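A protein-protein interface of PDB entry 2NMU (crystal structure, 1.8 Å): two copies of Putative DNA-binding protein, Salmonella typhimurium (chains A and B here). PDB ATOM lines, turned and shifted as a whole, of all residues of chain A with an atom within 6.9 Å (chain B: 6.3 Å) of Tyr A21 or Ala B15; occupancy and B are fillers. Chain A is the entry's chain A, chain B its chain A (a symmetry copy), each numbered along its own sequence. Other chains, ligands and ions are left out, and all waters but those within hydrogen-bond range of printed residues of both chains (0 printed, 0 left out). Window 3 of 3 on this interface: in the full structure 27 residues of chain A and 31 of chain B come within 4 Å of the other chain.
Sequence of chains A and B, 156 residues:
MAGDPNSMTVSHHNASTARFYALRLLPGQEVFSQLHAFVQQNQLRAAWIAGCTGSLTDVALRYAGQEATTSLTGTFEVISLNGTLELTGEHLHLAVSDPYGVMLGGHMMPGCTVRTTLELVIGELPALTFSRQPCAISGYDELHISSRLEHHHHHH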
ATOM      1  N   ARG A  19      28.279  23.940  -7.419  1.00  0.00           N
ATOM      2  CA  ARG A  19      26.895  24.088  -6.997  1.00  0.00           C
ATOM      3  C   ARG A  19      26.821  23.176  -5.778  1.00  0.00           C
ATOM      4  O   ARG A  19      27.336  22.057  -5.810  1.00  0.00           O
ATOM      5  CB  ARG A  19      25.936  23.598  -8.089  1.00  0.00           C
ATOM      6  CG  ARG A  19      24.461  23.787  -7.747  1.00  0.00           C
ATOM      7  CD  ARG A  19      23.555  23.524  -8.948  1.00  0.00           C
ATOM      8  NE  ARG A  19      23.628  22.141  -9.412  1.00  0.00           N
ATOM      9  CZ  ARG A  19      24.123  21.766 -10.588  1.00  0.00           C
ATOM     10  NH1 ARG A  19      24.594  22.673 -11.434  1.00  0.00           N
ATOM     11  NH2 ARG A  19      24.148  20.479 -10.917  1.00  0.00           N
ATOM     12  N   PHE A  20      26.192  23.641  -4.707  1.00  0.00           N
ATOM     13  CA  PHE A  20      26.114  22.844  -3.486  1.00  0.00           C
ATOM     14  C   PHE A  20      24.705  22.418  -3.104  1.00  0.00           C
ATOM     15  O   PHE A  20      23.726  23.118  -3.379  1.00  0.00           O
ATOM     16  CB  PHE A  20      26.752  23.623  -2.332  1.00  0.00           C
ATOM     17  CG  PHE A  20      28.236  23.812  -2.481  1.00  0.00           C
ATOM     18  CD1 PHE A  20      29.122  22.820  -2.064  1.00  0.00           C
ATOM     19  CD2 PHE A  20      28.750  24.953  -3.084  1.00  0.00           C
ATOM     20  CE1 PHE A  20      30.498  22.966  -2.253  1.00  0.00           C
ATOM     21  CE2 PHE A  20      30.128  25.107  -3.279  1.00  0.00           C
ATOM     22  CZ  PHE A  20      30.997  24.110  -2.863  1.00  0.00           C
ATOM     23  N   TYR A  21      24.613  21.255  -2.472  1.00  0.00           N
ATOM     24  CA  TYR A  21      23.338  20.718  -2.019  1.00  0.00           C
ATOM     25  C   TYR A  21      23.463  20.374  -0.548  1.00  0.00           C
ATOM     26  O   TYR A  21      24.504  19.892  -0.107  1.00  0.00           O
ATOM     27  CB  TYR A  21      22.980  19.434  -2.764  1.00  0.00           C
ATOM     28  CG  TYR A  21      22.859  19.573  -4.257  1.00  0.00           C
ATOM     29  CD1 TYR A  21      23.988  19.614  -5.067  1.00  0.00           C
ATOM     30  CD2 TYR A  21      21.609  19.641  -4.866  1.00  0.00           C
ATOM     31  CE1 TYR A  21      23.874  19.714  -6.457  1.00  0.00           C
ATOM     32  CE2 TYR A  21      21.484  19.743  -6.251  1.00  0.00           C
ATOM     33  CZ  TYR A  21      22.615  19.777  -7.036  1.00  0.00           C
ATOM     34  OH  TYR A  21      22.486  19.867  -8.397  1.00  0.00           O
ATOM     35  N   ALA A  22      22.407  20.622   0.216  1.00  0.00           N
ATOM     36  CA  ALA A  22      22.412  20.293   1.634  1.00  0.00           C
ATOM     37  C   ALA A  22      21.317  19.263   1.858  1.00  0.00           C
ATOM     38  O   ALA A  22      20.215  19.389   1.325  1.00  0.00           O
ATOM     39  CB  ALA A  22      22.151  21.539   2.474  1.00  0.00           C
ATOM     40  N   LEU A  23      21.615  18.227   2.626  1.00  0.00           N
ATOM     41  CA  LEU A  23      20.605  17.218   2.887  1.00  0.00           C
ATOM     42  C   LEU A  23      20.795  16.562   4.237  1.00  0.00           C
ATOM     43  O   LEU A  23      21.870  16.629   4.830  1.00  0.00           O
ATOM     44  CB  LEU A  23      20.602  16.147   1.790  1.00  0.00           C
ATOM     45  CG  LEU A  23      21.847  15.296   1.538  1.00  0.00           C
ATOM     46  CD1 LEU A  23      21.451  14.032   0.788  1.00  0.00           C
ATOM     47  CD2 LEU A  23      22.870  16.097   0.744  1.00  0.00           C
ATOM     48  N   PHE A  38      20.553  10.250  -4.344  1.00  0.00           N
ATOM     49  CA  PHE A  38      20.689  11.697  -4.498  1.00  0.00           C
ATOM     50  C   PHE A  38      21.448  12.017  -5.782  1.00  0.00           C
ATOM     51  O   PHE A  38      21.083  12.932  -6.522  1.00  0.00           O
ATOM     52  CB  PHE A  38      21.435  12.302  -3.309  1.00  0.00           C
ATOM     53  CG  PHE A  38      21.332  13.802  -3.235  1.00  0.00           C
ATOM     54  CD1 PHE A  38      20.166  14.408  -2.777  1.00  0.00           C
ATOM     55  CD2 PHE A  38      22.386  14.608  -3.647  1.00  0.00           C
ATOM     56  CE1 PHE A  38      20.049  15.797  -2.729  1.00  0.00           C
ATOM     57  CE2 PHE A  38      22.284  15.998  -3.605  1.00  0.00           C
ATOM     58  CZ  PHE A  38      21.113  16.594  -3.146  1.00  0.00           C
ATOM     59  N   ASN A  42      19.637  14.047  -9.027  1.00  0.00           N
ATOM     60  CA  ASN A  42      20.172  15.291  -9.553  1.00  0.00           C
ATOM     61  C   ASN A  42      21.166  15.104 -10.687  1.00  0.00           C
ATOM     62  O   ASN A  42      21.744  16.075 -11.173  1.00  0.00           O
ATOM     63  CB  ASN A  42      20.813  16.094  -8.424  1.00  0.00           C
ATOM     64  CG  ASN A  42      19.834  16.407  -7.319  1.00  0.00           C
ATOM     65  OD1 ASN A  42      19.765  15.700  -6.310  1.00  0.00           O
ATOM     66  ND2 ASN A  42      19.055  17.461  -7.508  1.00  0.00           N
ATOM     67  N   GLN A  43      21.345  13.858 -11.113  1.00  0.00           N
ATOM     68  CA  GLN A  43      22.271  13.532 -12.193  1.00  0.00           C
ATOM     69  C   GLN A  43      23.632  14.200 -12.001  1.00  0.00           C
ATOM     70  O   GLN A  43      24.150  14.858 -12.903  1.00  0.00           O
ATOM     71  CB  GLN A  43      21.665  13.944 -13.540  1.00  0.00           C
ATOM     72  CG  GLN A  43      20.418  13.145 -13.912  1.00  0.00           C
ATOM     73  CD  GLN A  43      20.732  11.707 -14.285  1.00  0.00           C
ATOM     74  OE1 GLN A  43      21.299  11.440 -15.343  1.00  0.00           O
ATOM     75  NE2 GLN A  43      20.372  10.774 -13.413  1.00  0.00           N
ATOM     76  N   LEU A  44      24.208  14.026 -10.816  1.00  0.00           N
ATOM     77  CA  LEU A  44      25.513  14.600 -10.512  1.00  0.00           C
ATOM     78  C   LEU A  44      26.602  13.817 -11.256  1.00  0.00           C
ATOM     79  O   LEU A  44      26.629  12.585 -11.218  1.00  0.00           O
ATOM     80  CB  LEU A  44      25.749  14.565  -9.000  1.00  0.00           C
ATOM     81  CG  LEU A  44      24.669  15.277  -8.173  1.00  0.00           C
ATOM     82  CD1 LEU A  44      25.049  15.258  -6.699  1.00  0.00           C
ATOM     83  CD2 LEU A  44      24.508  16.716  -8.664  1.00  0.00           C
ATOM     84  N   LEU A 120      24.738  16.483   5.405  1.00  0.00           N
ATOM     85  CA  LEU A 120      25.722  16.539   4.341  1.00  0.00           C
ATOM     86  C   LEU A 120      25.623  17.767   3.459  1.00  0.00           C
ATOM     87  O   LEU A 120      24.535  18.272   3.197  1.00  0.00           O
ATOM     88  CB  LEU A 120      25.564  15.321   3.429  1.00  0.00           C
ATOM     89  CG  LEU A 120      25.793  13.907   3.957  1.00  0.00           C
ATOM     90  CD1 LEU A 120      24.795  12.953   3.318  1.00  0.00           C
ATOM     91  CD2 LEU A 120      27.219  13.486   3.648  1.00  0.00           C
ATOM     92  N   VAL A 121      26.777  18.243   3.008  1.00  0.00           N
ATOM     93  CA  VAL A 121      26.820  19.346   2.064  1.00  0.00           C
ATOM     94  C   VAL A 121      27.616  18.713   0.935  1.00  0.00           C
ATOM     95  O   VAL A 121      28.772  18.331   1.116  1.00  0.00           O
ATOM     96  CB  VAL A 121      27.570  20.572   2.606  1.00  0.00           C
ATOM     97  CG1 VAL A 121      27.682  21.632   1.511  1.00  0.00           C
ATOM     98  CG2 VAL A 121      26.826  21.144   3.806  1.00  0.00           C
ATOM     99  N   ILE A 122      26.982  18.563  -0.219  1.00  0.00           N
ATOM    100  CA  ILE A 122      27.633  17.944  -1.357  1.00  0.00           C
ATOM    101  C   ILE A 122      27.872  18.966  -2.452  1.00  0.00           C
ATOM    102  O   ILE A 122      26.990  19.752  -2.783  1.00  0.00           O
ATOM    103  CB  ILE A 122      26.773  16.786  -1.902  1.00  0.00           C
ATOM    104  CG1 ILE A 122      26.652  15.696  -0.832  1.00  0.00           C
ATOM    105  CG2 ILE A 122      27.388  16.225  -3.181  1.00  0.00           C
ATOM    106  CD1 ILE A 122      25.676  14.586  -1.180  1.00  0.00           C
ATOM    107  N   GLY A 123      29.085  18.963  -2.989  1.00  0.00           N
ATOM    108  CA  GLY A 123      29.416  19.880  -4.060  1.00  0.00           C
ATOM    109  C   GLY A 123      29.409  19.149  -5.389  1.00  0.00           C
ATOM    110  O   GLY A 123      29.730  17.965  -5.452  1.00  0.00           O
ATOM    111  N   GLU A 124      29.013  19.857  -6.441  1.00  0.00           N
ATOM    112  CA  GLU A 124      28.977  19.319  -7.801  1.00  0.00           C
ATOM    113  C   GLU A 124      29.760  20.321  -8.657  1.00  0.00           C
ATOM    114  O   GLU A 124      29.597  21.527  -8.502  1.00  0.00           O
ATOM    115  CB  GLU A 124      27.531  19.212  -8.301  1.00  0.00           C
ATOM    116  CG  GLU A 124      27.401  19.092  -9.820  1.00  0.00           C
ATOM    117  CD  GLU A 124      27.762  17.718 -10.355  1.00  0.00           C
ATOM    118  OE1 GLU A 124      28.488  16.970  -9.670  1.00  0.00           O
ATOM    119  OE2 GLU A 124      27.327  17.387 -11.481  1.00  0.00           O
ATOM    120  N   HIS B  13      15.281  21.743  -4.665  1.00  0.00           N
ATOM    121  CA  HIS B  13      16.356  20.718  -4.804  1.00  0.00           C
ATOM    122  C   HIS B  13      17.405  20.912  -3.716  1.00  0.00           C
ATOM    123  O   HIS B  13      18.397  20.185  -3.659  1.00  0.00           O
ATOM    124  CB  HIS B  13      17.020  20.834  -6.180  1.00  0.00           C
ATOM    125  CG  HIS B  13      16.053  20.806  -7.322  1.00  0.00           C
ATOM    126  ND1 HIS B  13      15.201  19.747  -7.552  1.00  0.00           N
ATOM    127  CD2 HIS B  13      15.801  21.710  -8.299  1.00  0.00           C
ATOM    128  CE1 HIS B  13      14.466  20.001  -8.619  1.00  0.00           C
ATOM    129  NE2 HIS B  13      14.810  21.186  -9.092  1.00  0.00           N
ATOM    130  N   ASN B  14      17.175  21.896  -2.850  1.00  0.00           N
ATOM    131  CA  ASN B  14      18.103  22.205  -1.767  1.00  0.00           C
ATOM    132  C   ASN B  14      19.487  22.527  -2.324  1.00  0.00           C
ATOM    133  O   ASN B  14      20.501  22.248  -1.686  1.00  0.00           O
ATOM    134  CB  ASN B  14      18.202  21.028  -0.790  1.00  0.00           C
ATOM    135  CG  ASN B  14      16.901  20.765  -0.059  1.00  0.00           C
ATOM    136  OD1 ASN B  14      16.262  21.687   0.449  1.00  0.00           O
ATOM    137  ND2 ASN B  14      16.506  19.499   0.007  1.00  0.00           N
ATOM    138  N   ALA B  15      19.513  23.113  -3.519  1.00  0.00           N
ATOM    139  CA  ALA B  15      20.756  23.483  -4.190  1.00  0.00           C
ATOM    140  C   ALA B  15      21.049  24.959  -3.953  1.00  0.00           C
ATOM    141  O   ALA B  15      20.145  25.725  -3.623  1.00  0.00           O
ATOM    142  CB  ALA B  15      20.639  23.213  -5.682  1.00  0.00           C
ATOM    143  N   SER B  16      22.307  25.357  -4.129  1.00  0.00           N
ATOM    144  CA  SER B  16      22.688  26.749  -3.913  1.00  0.00           C
ATOM    145  C   SER B  16      24.135  27.034  -4.283  1.00  0.00           C
ATOM    146  O   SER B  16      24.970  26.129  -4.303  1.00  0.00           O
ATOM    147  CB  SER B  16      22.474  27.110  -2.437  1.00  0.00           C
ATOM    148  OG  SER B  16      23.026  28.382  -2.119  1.00  0.00           O
ATOM    149  N   THR B  17      24.431  28.291  -4.598  1.00  0.00           N
ATOM    150  CA  THR B  17      25.808  28.656  -4.878  1.00  0.00           C
ATOM    151  C   THR B  17      26.374  28.818  -3.469  1.00  0.00           C
ATOM    152  O   THR B  17      25.645  28.656  -2.489  1.00  0.00           O
ATOM    153  CB  THR B  17      25.919  30.003  -5.629  1.00  0.00           C
ATOM    154  OG1 THR B  17      25.290  31.040  -4.860  1.00  0.00           O
ATOM    155  CG2 THR B  17      25.254  29.908  -6.997  1.00  0.00           C
ATOM    156  N   LEU B 125      25.500  29.164   2.228  1.00  0.00           N
ATOM    157  CA  LEU B 125      24.644  28.850   1.082  1.00  0.00           C
ATOM    158  C   LEU B 125      23.514  29.877   1.041  1.00  0.00           C
ATOM    159  O   LEU B 125      22.478  29.690   1.670  1.00  0.00           O
ATOM    160  CB  LEU B 125      24.077  27.435   1.248  1.00  0.00           C
ATOM    161  CG  LEU B 125      25.142  26.337   1.394  1.00  0.00           C
ATOM    162  CD1 LEU B 125      24.513  25.060   1.933  1.00  0.00           C
ATOM    163  CD2 LEU B 125      25.799  26.087   0.047  1.00  0.00           C
ATOM    164  N   ALA B 127      21.103  30.605  -0.963  1.00  0.00           N
ATOM    165  CA  ALA B 127      19.759  30.206  -1.372  1.00  0.00           C
ATOM    166  C   ALA B 127      19.013  29.369  -0.342  1.00  0.00           C
ATOM    167  O   ALA B 127      17.818  29.095  -0.503  1.00  0.00           O
ATOM    168  CB  ALA B 127      19.827  29.451  -2.699  1.00  0.00           C
ATOM    169  N   LEU B 128      19.700  28.975   0.725  1.00  0.00           N
ATOM    170  CA  LEU B 128      19.080  28.142   1.747  1.00  0.00           C
ATOM    171  C   LEU B 128      19.099  28.744   3.146  1.00  0.00           C
ATOM    172  O   LEU B 128      19.763  29.746   3.404  1.00  0.00           O
ATOM    173  CB  LEU B 128      19.787  26.781   1.796  1.00  0.00           C
ATOM    174  CG  LEU B 128      19.916  26.017   0.477  1.00  0.00           C
ATOM    175  CD1 LEU B 128      20.791  24.787   0.693  1.00  0.00           C
ATOM    176  CD2 LEU B 128      18.537  25.617  -0.034  1.00  0.00           C
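N of Ala A22 sits at hydrogen-bond distance from O of Asn B14, at 3.1 Å.
The backbone carbonyl oxygen (O) of Phe A20 lies within hydrogen-bond range of the backbone NH (N) of Ser B16 (2.8 Å).
The backbone NH of Glu A124 sits at hydrogen-bond distance from the backbone carbonyl oxygen of Arg A19 (2.8 Å).
The side-chain hydroxyl (OH) of Tyr A21 is in hydrogen-bond range of the guanidinium group (NE) of Arg A19 (2.7 Å).
The backbone NH (N) of Ala B127 lies within hydrogen-bond range of the side-chain hydroxyl (OG) of Ser B16.
O of Tyr A21 sits at hydrogen-bond distance from N of Ile A122 (2.8 Å).
Hydrophobic or aromatic side chains of chain B that line the printed part of chain A: Ala B15, Leu B125 and Leu B128.
Along chain B the printed residues that touch a printed residue of chain A span positions 13 to 128.
Among the printed residues, 10 pairs touch across the chains.
Among the printed residues, no Asp or Glu carboxylate lies within 4 Å of a Lys or Arg side-chain nitrogen of the other chain.
Of chain A, only Phe A20 and Tyr A21 come within 4 Å of Ala B15.
Of the printed residues of chain B, Phe A20 touches Asn B14, Ala B15, Ser B16 and Leu B125.
Printed residues of chain A within 4 Å of Leu B128: Ala A22.
Printed residues of chain A within 4 Å of Asn B14: Phe A20 (3.7 Å), Tyr A21 (3.2 Å) and Ala A22 (3.1 Å).
Of the printed residues of chain B, Ala A22 touches Asn B14 (3.1 Å) and Leu B128 (3.9 Å).
Val A121 touches none of the printed residues of chain B.
Glu A124 touches none of the printed residues of chain B.
The nearest residue of chain B that does not touch Tyr A21 is Ser B16 (5.0 Å).
Among the printed residues, pairs that only touch across the chains: Phe A20 with Ala B15 (3.1 Å), Tyr A21 with Asn B14 (3.2 Å), Tyr A21 with His B13 (3.5 Å), Phe A20 with Leu B125 (3.6 Å), Tyr A21 with Ala B15 (3.6 Å), Phe A20 with Asn B14 (3.7 Å), Arg A19 with Ser B16 (3.8 Å) and Ala A22 with Leu B128 (3.9 Å).
No position is printed for both chains.
Of the 10 pairs that touch across the chains among the printed residues, none has its exchanged pair printed and touching as well.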
